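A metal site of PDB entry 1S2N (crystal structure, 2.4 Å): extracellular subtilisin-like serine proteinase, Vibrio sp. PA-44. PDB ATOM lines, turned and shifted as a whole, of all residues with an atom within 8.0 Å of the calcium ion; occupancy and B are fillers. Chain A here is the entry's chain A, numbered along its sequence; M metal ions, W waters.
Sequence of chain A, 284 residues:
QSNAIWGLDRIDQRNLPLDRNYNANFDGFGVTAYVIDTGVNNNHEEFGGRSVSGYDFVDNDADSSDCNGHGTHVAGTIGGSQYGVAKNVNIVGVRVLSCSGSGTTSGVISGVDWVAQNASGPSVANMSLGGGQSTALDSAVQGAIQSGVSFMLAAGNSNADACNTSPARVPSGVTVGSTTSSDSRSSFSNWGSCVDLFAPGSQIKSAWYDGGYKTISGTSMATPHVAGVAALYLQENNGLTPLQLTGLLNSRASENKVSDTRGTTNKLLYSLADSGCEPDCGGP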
ATOM      1  N   THR A  38     -18.805 -20.320 -10.543  1.00  0.00           N
ATOM      2  CA  THR A  38     -18.501 -20.764 -11.902  1.00  0.00           C
ATOM      3  C   THR A  38     -19.408 -21.920 -12.364  1.00  0.00           C
ATOM      4  O   THR A  38     -19.163 -22.527 -13.415  1.00  0.00           O
ATOM      5  CB  THR A  38     -17.023 -21.232 -12.007  1.00  0.00           C
ATOM      6  OG1 THR A  38     -16.789 -22.366 -11.162  1.00  0.00           O
ATOM      7  CG2 THR A  38     -16.048 -20.175 -11.485  1.00  0.00           C
ATOM      8  N   SER A  53     -29.078 -28.058 -11.772  1.00  0.00           N
ATOM      9  CA  SER A  53     -28.833 -26.773 -12.406  1.00  0.00           C
ATOM     10  C   SER A  53     -29.907 -25.762 -12.008  1.00  0.00           C
ATOM     11  O   SER A  53     -31.028 -26.149 -11.669  1.00  0.00           O
ATOM     12  CB  SER A  53     -28.774 -26.934 -13.935  1.00  0.00           C
ATOM     13  OG  SER A  53     -27.505 -27.426 -14.336  1.00  0.00           O
ATOM     14  N   TYR A  55     -29.632 -21.712 -13.281  1.00  0.00           N
ATOM     15  CA  TYR A  55     -29.461 -21.037 -14.563  1.00  0.00           C
ATOM     16  C   TYR A  55     -28.005 -20.651 -14.815  1.00  0.00           C
ATOM     17  O   TYR A  55     -27.216 -20.578 -13.887  1.00  0.00           O
ATOM     18  CB  TYR A  55     -30.356 -19.790 -14.667  1.00  0.00           C
ATOM     19  CG  TYR A  55     -30.604 -19.348 -16.087  1.00  0.00           C
ATOM     20  CD1 TYR A  55     -31.488 -20.026 -16.904  1.00  0.00           C
ATOM     21  CD2 TYR A  55     -29.932 -18.262 -16.627  1.00  0.00           C
ATOM     22  CE1 TYR A  55     -31.711 -19.626 -18.231  1.00  0.00           C
ATOM     23  CE2 TYR A  55     -30.132 -17.849 -17.942  1.00  0.00           C
ATOM     24  CZ  TYR A  55     -31.027 -18.534 -18.729  1.00  0.00           C
ATOM     25  OH  TYR A  55     -31.228 -18.131 -20.028  1.00  0.00           O
ATOM     26  N   ASP A  56     -27.676 -20.424 -16.078  1.00  0.00           N
ATOM     27  CA  ASP A  56     -26.335 -20.049 -16.503  1.00  0.00           C
ATOM     28  C   ASP A  56     -26.391 -18.673 -17.187  1.00  0.00           C
ATOM     29  O   ASP A  56     -26.822 -18.549 -18.327  1.00  0.00           O
ATOM     30  CB  ASP A  56     -25.793 -21.132 -17.471  1.00  0.00           C
ATOM     31  CG  ASP A  56     -24.420 -20.798 -18.041  1.00  0.00           C
ATOM     32  OD1 ASP A  56     -23.865 -21.661 -18.779  1.00  0.00           O
ATOM     33  OD2 ASP A  56     -23.812 -19.738 -17.822  1.00  0.00           O
ATOM     34  N   PHE A  57     -25.973 -17.644 -16.464  1.00  0.00           N
ATOM     35  CA  PHE A  57     -26.036 -16.261 -16.975  1.00  0.00           C
ATOM     36  C   PHE A  57     -24.821 -15.813 -17.770  1.00  0.00           C
ATOM     37  O   PHE A  57     -24.803 -14.711 -18.315  1.00  0.00           O
ATOM     38  CB  PHE A  57     -26.341 -15.304 -15.818  1.00  0.00           C
ATOM     39  CG  PHE A  57     -27.744 -15.412 -15.307  1.00  0.00           C
ATOM     40  CD1 PHE A  57     -28.797 -14.867 -16.029  1.00  0.00           C
ATOM     41  CD2 PHE A  57     -28.018 -16.100 -14.126  1.00  0.00           C
ATOM     42  CE1 PHE A  57     -30.100 -14.983 -15.563  1.00  0.00           C
ATOM     43  CE2 PHE A  57     -29.322 -16.217 -13.660  1.00  0.00           C
ATOM     44  CZ  PHE A  57     -30.363 -15.660 -14.386  1.00  0.00           C
ATOM     45  N   VAL A  58     -23.814 -16.685 -17.854  1.00  0.00           N
ATOM     46  CA  VAL A  58     -22.650 -16.446 -18.706  1.00  0.00           C
ATOM     47  C   VAL A  58     -22.968 -16.781 -20.164  1.00  0.00           C
ATOM     48  O   VAL A  58     -22.724 -15.978 -21.055  1.00  0.00           O
ATOM     49  CB  VAL A  58     -21.418 -17.277 -18.230  1.00  0.00           C
ATOM     50  CG1 VAL A  58     -20.214 -17.036 -19.150  1.00  0.00           C
ATOM     51  CG2 VAL A  58     -21.069 -16.936 -16.790  1.00  0.00           C
ATOM     52  N   ASP A  59     -23.532 -17.965 -20.388  1.00  0.00           N
ATOM     53  CA  ASP A  59     -23.863 -18.471 -21.732  1.00  0.00           C
ATOM     54  C   ASP A  59     -25.378 -18.437 -22.059  1.00  0.00           C
ATOM     55  O   ASP A  59     -25.782 -18.845 -23.152  1.00  0.00           O
ATOM     56  CB  ASP A  59     -23.341 -19.901 -21.886  1.00  0.00           C
ATOM     57  CG  ASP A  59     -21.815 -19.961 -21.994  1.00  0.00           C
ATOM     58  OD1 ASP A  59     -21.204 -19.021 -22.538  1.00  0.00           O
ATOM     59  OD2 ASP A  59     -21.147 -20.917 -21.549  1.00  0.00           O
ATOM     60  N   ASN A  60     -26.187 -17.958 -21.126  1.00  0.00           N
ATOM     61  CA  ASN A  60     -27.646 -17.911 -21.249  1.00  0.00           C
ATOM     62  C   ASN A  60     -28.274 -19.241 -21.658  1.00  0.00           C
ATOM     63  O   ASN A  60     -28.956 -19.326 -22.682  1.00  0.00           O
ATOM     64  CB  ASN A  60     -28.065 -16.790 -22.213  1.00  0.00           C
ATOM     65  CG  ASN A  60     -27.864 -15.422 -21.621  1.00  0.00           C
ATOM     66  OD1 ASN A  60     -28.216 -15.158 -20.469  1.00  0.00           O
ATOM     67  ND2 ASN A  60     -27.272 -14.528 -22.401  1.00  0.00           N
ATOM     68  N   ASP A  61     -28.007 -20.273 -20.864  1.00  0.00           N
ATOM     69  CA  ASP A  61     -28.621 -21.596 -21.052  1.00  0.00           C
ATOM     70  C   ASP A  61     -29.074 -22.200 -19.723  1.00  0.00           C
ATOM     71  O   ASP A  61     -28.883 -21.588 -18.669  1.00  0.00           O
ATOM     72  CB  ASP A  61     -27.663 -22.535 -21.820  1.00  0.00           C
ATOM     73  CG  ASP A  61     -26.366 -22.790 -21.079  1.00  0.00           C
ATOM     74  OD1 ASP A  61     -26.404 -23.162 -19.899  1.00  0.00           O
ATOM     75  OD2 ASP A  61     -25.242 -22.653 -21.607  1.00  0.00           O
ATOM     76  N   ALA A  62     -29.676 -23.378 -19.766  1.00  0.00           N
ATOM     77  CA  ALA A  62     -30.265 -24.006 -18.571  1.00  0.00           C
ATOM     78  C   ALA A  62     -29.304 -24.918 -17.822  1.00  0.00           C
ATOM     79  O   ALA A  62     -29.665 -25.486 -16.785  1.00  0.00           O
ATOM     80  CB  ALA A  62     -31.531 -24.783 -18.956  1.00  0.00           C
ATOM     81  N   ASP A  63     -28.089 -25.064 -18.347  1.00  0.00           N
ATOM     82  CA  ASP A  63     -27.091 -25.980 -17.801  1.00  0.00           C
ATOM     83  C   ASP A  63     -25.982 -25.207 -17.084  1.00  0.00           C
ATOM     84  O   ASP A  63     -25.075 -24.663 -17.720  1.00  0.00           O
ATOM     85  CB  ASP A  63     -26.519 -26.837 -18.931  1.00  0.00           C
ATOM     86  CG  ASP A  63     -25.655 -27.981 -18.413  1.00  0.00           C
ATOM     87  OD1 ASP A  63     -25.459 -28.955 -19.158  1.00  0.00           O
ATOM     88  OD2 ASP A  63     -25.136 -27.983 -17.294  1.00  0.00           O
ATOM     89  N   SER A  64     -26.052 -25.174 -15.760  1.00  0.00           N
ATOM     90  CA  SER A  64     -25.081 -24.455 -14.933  1.00  0.00           C
ATOM     91  C   SER A  64     -23.867 -25.326 -14.556  1.00  0.00           C
ATOM     92  O   SER A  64     -23.296 -25.171 -13.484  1.00  0.00           O
ATOM     93  CB  SER A  64     -25.776 -23.910 -13.671  1.00  0.00           C
ATOM     94  OG  SER A  64     -26.238 -24.957 -12.837  1.00  0.00           O
ATOM     95  N   SER A  65     -23.458 -26.210 -15.464  1.00  0.00           N
ATOM     96  CA  SER A  65     -22.307 -27.090 -15.242  1.00  0.00           C
ATOM     97  C   SER A  65     -21.046 -26.259 -15.062  1.00  0.00           C
ATOM     98  O   SER A  65     -20.902 -25.192 -15.656  1.00  0.00           O
ATOM     99  CB  SER A  65     -22.126 -28.057 -16.427  1.00  0.00           C
ATOM    100  OG  SER A  65     -23.154 -29.035 -16.458  1.00  0.00           O
ATOM    101  N   ASP A  66     -20.119 -26.775 -14.246  1.00  0.00           N
ATOM    102  CA  ASP A  66     -18.869 -26.108 -13.911  1.00  0.00           C
ATOM    103  C   ASP A  66     -17.738 -26.529 -14.840  1.00  0.00           C
ATOM    104  O   ASP A  66     -17.494 -27.718 -15.002  1.00  0.00           O
ATOM    105  CB  ASP A  66     -18.500 -26.478 -12.481  1.00  0.00           C
ATOM    106  CG  ASP A  66     -17.390 -25.617 -11.897  1.00  0.00           C
ATOM    107  OD1 ASP A  66     -17.110 -24.518 -12.423  1.00  0.00           O
ATOM    108  OD2 ASP A  66     -16.742 -25.974 -10.892  1.00  0.00           O
ATOM    109  N   CYS A  67     -17.032 -25.560 -15.430  1.00  0.00           N
ATOM    110  CA  CYS A  67     -15.840 -25.838 -16.260  1.00  0.00           C
ATOM    111  C   CYS A  67     -14.607 -25.093 -15.766  1.00  0.00           C
ATOM    112  O   CYS A  67     -13.627 -24.956 -16.497  1.00  0.00           O
ATOM    113  CB  CYS A  67     -16.105 -25.514 -17.735  1.00  0.00           C
ATOM    114  SG  CYS A  67     -16.720 -23.842 -17.993  1.00  0.00           S
ATOM    115  N   ARG A  95     -24.678 -20.190 -12.408  1.00  0.00           N
ATOM    116  CA  ARG A  95     -23.410 -19.882 -13.062  1.00  0.00           C
ATOM    117  C   ARG A  95     -23.309 -18.413 -13.539  1.00  0.00           C
ATOM    118  O   ARG A  95     -23.956 -18.047 -14.503  1.00  0.00           O
ATOM    119  CB  ARG A  95     -23.187 -20.839 -14.237  1.00  0.00           C
ATOM    120  CG  ARG A  95     -21.861 -20.684 -14.964  1.00  0.00           C
ATOM    121  CD  ARG A  95     -21.390 -21.932 -15.687  1.00  0.00           C
ATOM    122  NE  ARG A  95     -20.104 -21.713 -16.338  1.00  0.00           N
ATOM    123  CZ  ARG A  95     -19.944 -21.255 -17.584  1.00  0.00           C
ATOM    124  NH1 ARG A  95     -18.712 -21.078 -18.052  1.00  0.00           N
ATOM    125  NH2 ARG A  95     -20.977 -20.993 -18.359  1.00  0.00           N
HETATM  126 CA    CA M   1     -24.001 -23.840 -19.515  1.00  0.00          CA
HETATM  127  O   HOH W   1     -22.398 -23.018 -21.029  1.00  0.00           O
HETATM  128  O   HOH W   2     -23.384 -26.144 -20.813  1.00  0.00           O
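OD2 of Asp 63 sits at hydrogen-bond distance from N of Ser 65 (3.1 Å). OD2 of Asp 56 lies within salt-bridge range of NH2 of Arg 95 (3.1 Å). The side-chain carboxylate (OD2) of Asp 56 sits at hydrogen-bond distance from the backbone NH (N) of Asp 59 (3.1 Å). The backbone NH (N) of Val 58 lies within hydrogen-bond range of the side-chain carboxylate (OD2) of Asp 56, at 3.1 Å.
The calcium ion is bound by O of Asp 63 (2.2 Å), OD1 of Asp 56 (2.3 Å), water W1 (2.4 Å), OD1 of Asp 61 (2.5 Å), OD2 of Asp 61 (2.7 Å) and water W2 (2.7 Å). The calcium ion has six donor atoms within binding distance.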
